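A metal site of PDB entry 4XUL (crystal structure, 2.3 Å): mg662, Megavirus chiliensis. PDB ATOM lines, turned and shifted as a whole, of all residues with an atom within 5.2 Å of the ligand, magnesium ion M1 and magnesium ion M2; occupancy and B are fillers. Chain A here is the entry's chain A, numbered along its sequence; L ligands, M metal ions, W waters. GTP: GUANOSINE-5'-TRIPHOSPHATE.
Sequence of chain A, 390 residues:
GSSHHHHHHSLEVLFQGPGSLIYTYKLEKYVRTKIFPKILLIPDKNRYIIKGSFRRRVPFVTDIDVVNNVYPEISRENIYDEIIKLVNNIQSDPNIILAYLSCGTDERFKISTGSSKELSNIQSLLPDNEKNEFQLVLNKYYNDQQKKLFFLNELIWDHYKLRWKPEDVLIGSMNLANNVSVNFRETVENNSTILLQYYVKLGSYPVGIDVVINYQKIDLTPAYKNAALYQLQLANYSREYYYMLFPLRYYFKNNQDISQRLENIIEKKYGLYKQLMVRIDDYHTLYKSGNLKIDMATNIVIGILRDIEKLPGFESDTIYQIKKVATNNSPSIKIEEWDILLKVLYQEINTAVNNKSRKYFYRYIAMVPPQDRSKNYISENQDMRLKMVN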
ATOM      1  N   GLY A  52       9.010  15.594  -4.002  1.00  0.00           N
ATOM      2  CA  GLY A  52      10.243  15.456  -4.768  1.00  0.00           C
ATOM      3  C   GLY A  52      11.492  15.828  -3.994  1.00  0.00           C
ATOM      4  O   GLY A  52      11.532  15.782  -2.769  1.00  0.00           O
ATOM      5  N   SER A  53      12.530  16.218  -4.733  1.00  0.00           N
ATOM      6  CA  SER A  53      13.848  16.433  -4.149  1.00  0.00           C
ATOM      7  C   SER A  53      13.950  17.698  -3.298  1.00  0.00           C
ATOM      8  O   SER A  53      14.809  17.779  -2.422  1.00  0.00           O
ATOM      9  CB  SER A  53      14.903  16.460  -5.253  1.00  0.00           C
ATOM     10  OG  SER A  53      14.633  17.500  -6.177  1.00  0.00           O
ATOM     11  N   ARG A  56      13.233  16.976   0.191  1.00  0.00           N
ATOM     12  CA  ARG A  56      14.365  16.335   0.836  1.00  0.00           C
ATOM     13  C   ARG A  56      15.536  17.306   0.977  1.00  0.00           C
ATOM     14  O   ARG A  56      16.601  16.941   1.478  1.00  0.00           O
ATOM     15  CB  ARG A  56      14.806  15.095   0.051  1.00  0.00           C
ATOM     16  CG  ARG A  56      13.823  13.931   0.109  1.00  0.00           C
ATOM     17  CD  ARG A  56      14.456  12.652  -0.406  1.00  0.00           C
ATOM     18  NE  ARG A  56      15.139  12.870  -1.683  1.00  0.00           N
ATOM     19  CZ  ARG A  56      14.532  12.841  -2.863  1.00  0.00           C
ATOM     20  NH1 ARG A  56      13.236  12.597  -2.935  1.00  0.00           N
ATOM     21  NH2 ARG A  56      15.223  13.046  -3.973  1.00  0.00           N
ATOM     22  N   VAL A  58      17.672  18.607  -1.145  1.00  0.00           N
ATOM     23  CA  VAL A  58      18.915  18.199  -1.790  1.00  0.00           C
ATOM     24  C   VAL A  58      19.754  19.425  -2.155  1.00  0.00           C
ATOM     25  O   VAL A  58      19.211  20.466  -2.530  1.00  0.00           O
ATOM     26  CB  VAL A  58      18.646  17.323  -3.041  1.00  0.00           C
ATOM     27  CG1 VAL A  58      17.728  16.167  -2.683  1.00  0.00           C
ATOM     28  CG2 VAL A  58      18.052  18.149  -4.178  1.00  0.00           C
ATOM     29  N   THR A  62      17.184  21.148  -8.316  1.00  0.00           N
ATOM     30  CA  THR A  62      16.793  20.885  -9.694  1.00  0.00           C
ATOM     31  C   THR A  62      15.523  21.654 -10.036  1.00  0.00           C
ATOM     32  O   THR A  62      15.539  22.570 -10.849  1.00  0.00           O
ATOM     33  CB  THR A  62      16.557  19.390  -9.940  1.00  0.00           C
ATOM     34  OG1 THR A  62      15.584  18.901  -9.014  1.00  0.00           O
ATOM     35  CG2 THR A  62      17.857  18.610  -9.781  1.00  0.00           C
ATOM     36  N   ASP A  63      14.426  21.269  -9.394  1.00  0.00           N
ATOM     37  CA  ASP A  63      13.169  21.991  -9.533  1.00  0.00           C
ATOM     38  C   ASP A  63      12.392  21.909  -8.233  1.00  0.00           C
ATOM     39  O   ASP A  63      12.872  21.354  -7.253  1.00  0.00           O
ATOM     40  CB  ASP A  63      12.353  21.439 -10.713  1.00  0.00           C
ATOM     41  CG  ASP A  63      11.876  20.013 -10.483  1.00  0.00           C
ATOM     42  OD1 ASP A  63      12.407  19.314  -9.589  1.00  0.00           O
ATOM     43  OD2 ASP A  63      10.968  19.576 -11.216  1.00  0.00           O
ATOM     44  N   ILE A  64      11.189  22.466  -8.231  1.00  0.00           N
ATOM     45  CA  ILE A  64      10.322  22.378  -7.060  1.00  0.00           C
ATOM     46  C   ILE A  64       8.976  21.795  -7.457  1.00  0.00           C
ATOM     47  O   ILE A  64       8.318  22.292  -8.367  1.00  0.00           O
ATOM     48  CB  ILE A  64      10.126  23.766  -6.397  1.00  0.00           C
ATOM     49  CG1 ILE A  64      11.476  24.413  -6.082  1.00  0.00           C
ATOM     50  CG2 ILE A  64       9.299  23.628  -5.120  1.00  0.00           C
ATOM     51  CD1 ILE A  64      11.370  25.793  -5.481  1.00  0.00           C
ATOM     52  N   ASP A  65       8.583  20.725  -6.765  1.00  0.00           N
ATOM     53  CA  ASP A  65       7.351  20.018  -7.104  1.00  0.00           C
ATOM     54  C   ASP A  65       6.321  20.199  -5.987  1.00  0.00           C
ATOM     55  O   ASP A  65       6.614  19.904  -4.817  1.00  0.00           O
ATOM     56  CB  ASP A  65       7.645  18.536  -7.352  1.00  0.00           C
ATOM     57  CG  ASP A  65       8.805  18.323  -8.317  1.00  0.00           C
ATOM     58  OD1 ASP A  65       8.587  18.372  -9.544  1.00  0.00           O
ATOM     59  OD2 ASP A  65       9.941  18.105  -7.835  1.00  0.00           O
ATOM     60  N   ASP A 210       6.907  22.841 -10.687  1.00  0.00           N
ATOM     61  CA  ASP A 210       5.766  22.063 -11.142  1.00  0.00           C
ATOM     62  C   ASP A 210       4.669  22.046 -10.077  1.00  0.00           C
ATOM     63  O   ASP A 210       4.883  21.573  -8.960  1.00  0.00           O
ATOM     64  CB  ASP A 210       6.193  20.624 -11.475  1.00  0.00           C
ATOM     65  CG  ASP A 210       7.177  20.553 -12.625  1.00  0.00           C
ATOM     66  OD1 ASP A 210       7.131  21.438 -13.501  1.00  0.00           O
ATOM     67  OD2 ASP A 210       8.010  19.623 -12.640  1.00  0.00           O
ATOM     68  N   GLN A 231       9.697   5.781 -14.146  1.00  0.00           N
ATOM     69  CA  GLN A 231      11.077   6.211 -13.999  1.00  0.00           C
ATOM     70  C   GLN A 231      12.010   4.996 -13.989  1.00  0.00           C
ATOM     71  O   GLN A 231      13.098   5.045 -14.568  1.00  0.00           O
ATOM     72  CB  GLN A 231      11.241   7.047 -12.730  1.00  0.00           C
ATOM     73  CG  GLN A 231      12.561   7.801 -12.622  1.00  0.00           C
ATOM     74  CD  GLN A 231      13.679   6.930 -12.095  1.00  0.00           C
ATOM     75  OE1 GLN A 231      13.440   6.013 -11.306  1.00  0.00           O
ATOM     76  NE2 GLN A 231      14.905   7.212 -12.515  1.00  0.00           N
ATOM     77  N   LEU A 234      12.177   3.775 -17.641  1.00  0.00           N
ATOM     78  CA  LEU A 234      12.944   4.723 -18.430  1.00  0.00           C
ATOM     79  C   LEU A 234      14.449   4.550 -18.215  1.00  0.00           C
ATOM     80  O   LEU A 234      15.222   4.510 -19.171  1.00  0.00           O
ATOM     81  CB  LEU A 234      12.536   6.153 -18.084  1.00  0.00           C
ATOM     82  CG  LEU A 234      13.319   7.258 -18.809  1.00  0.00           C
ATOM     83  CD1 LEU A 234      13.143   7.149 -20.315  1.00  0.00           C
ATOM     84  CD2 LEU A 234      12.897   8.634 -18.308  1.00  0.00           C
ATOM     85  N   ALA A 235      14.844   4.432 -16.957  1.00  0.00           N
ATOM     86  CA  ALA A 235      16.255   4.296 -16.601  1.00  0.00           C
ATOM     87  C   ALA A 235      16.818   2.957 -17.060  1.00  0.00           C
ATOM     88  O   ALA A 235      17.892   2.893 -17.653  1.00  0.00           O
ATOM     89  CB  ALA A 235      16.434   4.478 -15.101  1.00  0.00           C
ATOM     90  N   GLU A 240      20.684   3.534 -18.007  1.00  0.00           N
ATOM     91  CA  GLU A 240      21.245   4.704 -17.353  1.00  0.00           C
ATOM     92  C   GLU A 240      21.440   4.419 -15.860  1.00  0.00           C
ATOM     93  O   GLU A 240      20.556   4.676 -15.049  1.00  0.00           O
ATOM     94  CB  GLU A 240      20.348   5.914 -17.575  1.00  0.00           C
ATOM     95  CG  GLU A 240      20.272   6.345 -19.032  1.00  0.00           C
ATOM     96  CD  GLU A 240      19.145   7.321 -19.301  1.00  0.00           C
ATOM     97  OE1 GLU A 240      18.109   7.225 -18.623  1.00  0.00           O
ATOM     98  OE2 GLU A 240      19.290   8.168 -20.210  1.00  0.00           O
ATOM     99  N   TYR A 243      20.385   6.825 -12.955  1.00  0.00           N
ATOM    100  CA  TYR A 243      18.956   6.920 -12.685  1.00  0.00           C
ATOM    101  C   TYR A 243      18.377   5.589 -12.232  1.00  0.00           C
ATOM    102  O   TYR A 243      17.339   5.558 -11.575  1.00  0.00           O
ATOM    103  CB  TYR A 243      18.235   7.453 -13.917  1.00  0.00           C
ATOM    104  CG  TYR A 243      18.597   8.898 -14.193  1.00  0.00           C
ATOM    105  CD1 TYR A 243      18.166   9.906 -13.343  1.00  0.00           C
ATOM    106  CD2 TYR A 243      19.372   9.237 -15.289  1.00  0.00           C
ATOM    107  CE1 TYR A 243      18.501  11.218 -13.577  1.00  0.00           C
ATOM    108  CE2 TYR A 243      19.718  10.562 -15.528  1.00  0.00           C
ATOM    109  CZ  TYR A 243      19.275  11.545 -14.665  1.00  0.00           C
ATOM    110  OH  TYR A 243      19.606  12.866 -14.887  1.00  0.00           O
ATOM    111  N   PHE A 246      17.671   5.301  -8.548  1.00  0.00           N
ATOM    112  CA  PHE A 246      16.482   5.921  -7.966  1.00  0.00           C
ATOM    113  C   PHE A 246      15.492   4.887  -7.394  1.00  0.00           C
ATOM    114  O   PHE A 246      15.032   5.063  -6.263  1.00  0.00           O
ATOM    115  CB  PHE A 246      15.769   6.805  -8.996  1.00  0.00           C
ATOM    116  CG  PHE A 246      16.415   8.151  -9.199  1.00  0.00           C
ATOM    117  CD1 PHE A 246      17.780   8.277  -9.372  1.00  0.00           C
ATOM    118  CD2 PHE A 246      15.639   9.301  -9.224  1.00  0.00           C
ATOM    119  CE1 PHE A 246      18.361   9.519  -9.558  1.00  0.00           C
ATOM    120  CE2 PHE A 246      16.210  10.542  -9.413  1.00  0.00           C
ATOM    121  CZ  PHE A 246      17.575  10.656  -9.577  1.00  0.00           C
ATOM    122  N   GLU A 267      22.648  12.609  -4.726  1.00  0.00           N
ATOM    123  CA  GLU A 267      22.434  14.044  -4.560  1.00  0.00           C
ATOM    124  C   GLU A 267      23.710  14.842  -4.309  1.00  0.00           C
ATOM    125  O   GLU A 267      23.781  16.018  -4.664  1.00  0.00           O
ATOM    126  CB  GLU A 267      21.435  14.289  -3.434  1.00  0.00           C
ATOM    127  CG  GLU A 267      20.103  13.550  -3.584  1.00  0.00           C
ATOM    128  CD  GLU A 267      19.290  14.004  -4.791  1.00  0.00           C
ATOM    129  OE1 GLU A 267      19.656  14.995  -5.462  1.00  0.00           O
ATOM    130  OE2 GLU A 267      18.253  13.360  -5.070  1.00  0.00           O
ATOM    131  N   LYS A 274      23.151  15.667 -12.362  1.00  0.00           N
ATOM    132  CA  LYS A 274      21.699  15.691 -12.476  1.00  0.00           C
ATOM    133  C   LYS A 274      21.204  17.117 -12.696  1.00  0.00           C
ATOM    134  O   LYS A 274      20.366  17.355 -13.561  1.00  0.00           O
ATOM    135  CB  LYS A 274      21.051  15.075 -11.232  1.00  0.00           C
ATOM    136  CG  LYS A 274      19.529  15.217 -11.175  1.00  0.00           C
ATOM    137  CD  LYS A 274      18.861  14.211 -10.225  1.00  0.00           C
ATOM    138  CE  LYS A 274      19.417  14.300  -8.806  1.00  0.00           C
ATOM    139  NZ  LYS A 274      19.012  15.554  -8.083  1.00  0.00           N
ATOM    140  N   VAL A 278      19.056  18.749 -15.892  1.00  0.00           N
ATOM    141  CA  VAL A 278      17.788  19.455 -15.711  1.00  0.00           C
ATOM    142  C   VAL A 278      17.851  20.867 -16.297  1.00  0.00           C
ATOM    143  O   VAL A 278      16.928  21.320 -16.977  1.00  0.00           O
ATOM    144  CB  VAL A 278      17.381  19.528 -14.230  1.00  0.00           C
ATOM    145  CG1 VAL A 278      16.222  20.493 -14.028  1.00  0.00           C
ATOM    146  CG2 VAL A 278      17.030  18.141 -13.710  1.00  0.00           C
ATOM    147  N   ASP A 281      17.642  20.755 -19.968  1.00  0.00           N
ATOM    148  CA  ASP A 281      16.272  20.442 -20.353  1.00  0.00           C
ATOM    149  C   ASP A 281      15.421  21.712 -20.229  1.00  0.00           C
ATOM    150  O   ASP A 281      14.579  21.979 -21.089  1.00  0.00           O
ATOM    151  CB  ASP A 281      15.708  19.328 -19.471  1.00  0.00           C
ATOM    152  CG  ASP A 281      15.483  18.043 -20.240  1.00  0.00           C
ATOM    153  OD1 ASP A 281      15.196  18.109 -21.450  1.00  0.00           O
ATOM    154  OD2 ASP A 281      15.582  16.959 -19.628  1.00  0.00           O
ATOM    155  N   TYR A 346      24.150  17.242 -23.168  1.00  0.00           N
ATOM    156  CA  TYR A 346      23.272  16.525 -22.260  1.00  0.00           C
ATOM    157  C   TYR A 346      23.607  15.029 -22.229  1.00  0.00           C
ATOM    158  O   TYR A 346      23.725  14.437 -21.167  1.00  0.00           O
ATOM    159  CB  TYR A 346      21.802  16.730 -22.660  1.00  0.00           C
ATOM    160  CG  TYR A 346      20.793  15.989 -21.799  1.00  0.00           C
ATOM    161  CD1 TYR A 346      20.501  14.646 -22.021  1.00  0.00           C
ATOM    162  CD2 TYR A 346      20.108  16.647 -20.782  1.00  0.00           C
ATOM    163  CE1 TYR A 346      19.581  13.974 -21.251  1.00  0.00           C
ATOM    164  CE2 TYR A 346      19.175  15.981 -20.004  1.00  0.00           C
ATOM    165  CZ  TYR A 346      18.917  14.645 -20.237  1.00  0.00           C
ATOM    166  OH  TYR A 346      17.996  13.982 -19.466  1.00  0.00           O
ATOM    167  N   ASN A 350      25.125  12.747 -19.390  1.00  0.00           N
ATOM    168  CA  ASN A 350      24.366  11.549 -19.063  1.00  0.00           C
ATOM    169  C   ASN A 350      25.250  10.295 -19.124  1.00  0.00           C
ATOM    170  O   ASN A 350      25.214   9.447 -18.230  1.00  0.00           O
ATOM    171  CB  ASN A 350      23.170  11.416 -20.021  1.00  0.00           C
ATOM    172  CG  ASN A 350      22.147  10.410 -19.536  1.00  0.00           C
ATOM    173  OD1 ASN A 350      21.999  10.175 -18.339  1.00  0.00           O
ATOM    174  ND2 ASN A 350      21.417   9.816 -20.473  1.00  0.00           N
HETATM  175  PG  GTP L   1      10.658  14.950 -10.510  1.00  0.00           P
HETATM  176  O1G GTP L   1      11.028  16.418 -10.361  1.00  0.00           O
HETATM  177  O2G GTP L   1      10.757  14.465 -11.944  1.00  0.00           O
HETATM  178  O3G GTP L   1       9.379  14.568  -9.808  1.00  0.00           O
HETATM  179  O3B GTP L   1      11.834  14.126  -9.751  1.00  0.00           O
HETATM  180  PB  GTP L   1      12.375  14.416  -8.247  1.00  0.00           P
HETATM  181  O1B GTP L   1      11.960  15.796  -7.775  1.00  0.00           O
HETATM  182  O2B GTP L   1      12.016  13.215  -7.392  1.00  0.00           O
HETATM  183  O3A GTP L   1      13.978  14.342  -8.481  1.00  0.00           O
HETATM  184  PA  GTP L   1      14.813  15.590  -9.073  1.00  0.00           P
HETATM  185  O1A GTP L   1      13.884  16.735  -9.378  1.00  0.00           O
HETATM  186  O2A GTP L   1      16.035  15.822  -8.216  1.00  0.00           O
HETATM  187  O5' GTP L   1      15.305  14.956 -10.468  1.00  0.00           O
HETATM  188  C5' GTP L   1      14.370  14.912 -11.544  1.00  0.00           C
HETATM  189  C4' GTP L   1      15.084  15.059 -12.868  1.00  0.00           C
HETATM  190  O4' GTP L   1      15.913  13.928 -13.129  1.00  0.00           O
HETATM  191  C3' GTP L   1      14.077  15.135 -14.003  1.00  0.00           C
HETATM  192  O3' GTP L   1      13.827  16.498 -14.372  1.00  0.00           O
HETATM  193  C2' GTP L   1      14.744  14.401 -15.153  1.00  0.00           C
HETATM  194  O2' GTP L   1      15.318  15.381 -16.015  1.00  0.00           O
HETATM  195  C1' GTP L   1      15.856  13.585 -14.513  1.00  0.00           C
HETATM  196  N9  GTP L   1      15.600  12.125 -14.663  1.00  0.00           N
HETATM  197  C8  GTP L   1      14.962  11.346 -13.770  1.00  0.00           C
HETATM  198  N7  GTP L   1      14.906  10.058 -14.195  1.00  0.00           N
HETATM  199  C5  GTP L   1      15.536  10.000 -15.389  1.00  0.00           C
HETATM  200  C6  GTP L   1      15.845   8.943 -16.383  1.00  0.00           C
HETATM  201  O6  GTP L   1      15.489   7.758 -16.204  1.00  0.00           O
HETATM  202  N1  GTP L   1      16.508   9.297 -17.493  1.00  0.00           N
HETATM  203  C2  GTP L   1      16.906  10.566 -17.709  1.00  0.00           C
HETATM  204  N2  GTP L   1      17.584  10.855 -18.848  1.00  0.00           N
HETATM  205  N3  GTP L   1      16.658  11.579 -16.844  1.00  0.00           N
HETATM  206  C4  GTP L   1      15.987  11.361 -15.689  1.00  0.00           C
HETATM  207 MG    MG M   1       9.481  18.128 -11.365  1.00  0.00          MG
HETATM  208 MG    MG M   2      11.870  17.559  -8.838  1.00  0.00          MG
HETATM  209  O   HOH W   1      13.112  17.950 -12.581  1.00  0.00           O
HETATM  210  O   HOH W   2      12.193  11.842 -11.907  1.00  0.00           O
HETATM  211  O   HOH W   3      16.215  13.183  -6.715  1.00  0.00           O
HETATM  212  O   HOH W   4      10.361  17.237 -13.474  1.00  0.00           O
HETATM  213  O   HOH W   5      12.781  18.524  -7.224  1.00  0.00           O
HETATM  214  O   HOH W   6       8.179  16.511 -11.782  1.00  0.00           O
HETATM  215  O   HOH W   7       7.955  14.845  -7.579  1.00  0.00           O
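An oxygen (O2A) of the ligand lies within hydrogen-bond range of the side-chain hydroxyl (OG) of Ser 53 (3.0 Å). NE2 of Gln 231 lies within hydrogen-bond range of N7 of the ligand, at 3.3 Å. OE1 of Glu 240 is in hydrogen-bond range of N1 of the ligand (2.9 Å). OG1 of Thr 62 sits at hydrogen-bond distance from O2A of the ligand (3.2 Å). The backbone NH of Ala 235 sits at hydrogen-bond distance from an oxygen (O6) of the ligand. The side-chain amino group (NZ) of Lys 274 is in salt-bridge range of an oxygen (O2A) of the ligand, at 3.0 Å. The backbone NH of Ser 53 lies close to an oxygen (O1B) of the ligand. The side-chain hydroxyl of Tyr 346 is in hydrogen-bond range of a nitrogen (N2) of the ligand (3.2 Å).
The side-chain carboxylate (OE2) of Glu 240 is in hydrogen-bond range of the side-chain amide nitrogen (ND2) of Asn 350 (2.7 Å). The side-chain amino group of Lys 274 is in salt-bridge range of the side-chain carboxylate of Glu 267, at 2.8 Å. The backbone NH (N) of Glu 240 is in hydrogen-bond range of the backbone carbonyl oxygen (O) of Ala 235 (2.9 Å). O of Ile 64 sits at hydrogen-bond distance from N of Asp 210 (2.8 Å). The backbone carbonyl oxygen of Ser 53 sits at hydrogen-bond distance from the backbone NH of Val 58. O of Tyr 243 is in hydrogen-bond range of NE2 of Gln 231, at 3.1 Å. OG1 of Thr 62 sits at hydrogen-bond distance from OG of Ser 53. The side-chain hydroxyl (OG1) of Thr 62 sits close to the side-chain carboxylate (OD1) of Asp 63, at 3.3 Å.
Gly 52 touches the ligand (CA to O1B, 3.5 Å). CG of Leu 234 touches O6 of the ligand, at 3.4 Å. Tyr 243 touches the ligand. Val 278 touches the ligand. Asp 281 touches the ligand (OD2 to O2', 3.95 Å). Hydrophobic or aromatic side chains that line the ligand: Leu 234, Ala 235, Tyr 243 and Val 278.
Three residues have an atom within 4 Å of magnesium ion M1: Asp 63, Asp 65 and Asp 210.
OG of Ser 53 touches magnesium ion M2, at 3.8 Å. Thr 62 touches magnesium ion M2 (OG1 to MG, 3.95 Å). Within 4 Å of magnesium ion M2: Ser 53, Thr 62, Asp 63 and Asp 65. The nearest printed residue that does not touch magnesium ion M2 is Gly 52 (4.9 Å).
Magnesium ion M1 is bound by the side-chain carboxylate (OD1) of Asp 65, the side-chain carboxylate (OD2) of Asp 63, water W6, water W4, the side-chain carboxylate (OD2) of Asp 210 and an oxygen (O1G) of the ligand.
Magnesium ion M2 is bound by OD1 of Asp 63, 2.0 Å away. An oxygen (O1B) of the ligand binds magnesium ion M2. An oxygen (O1G) of the ligand binds magnesium ion M2 (2.1 Å). Magnesium ion M2 is bound by water W5 (2.1 Å). OD2 of Asp 65 binds magnesium ion M2, 2.2 Å away. Magnesium ion M2 is bound by O1A of the ligand, at 2.2 Å. Magnesium ion M2 has six donor atoms within binding distance.
Water W5 lies within hydrogen-bond range of O of Asp 63 (2.8 Å), OG1 of Thr 62 (3.3 Å) and N of Ser 53 (3.4 Å). Water W3 lies within hydrogen-bond range of OE2 of Glu 267 (2.6 Å), NH2 of Arg 56 (2.9 Å) and O2A of the ligand (3.0 Å).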
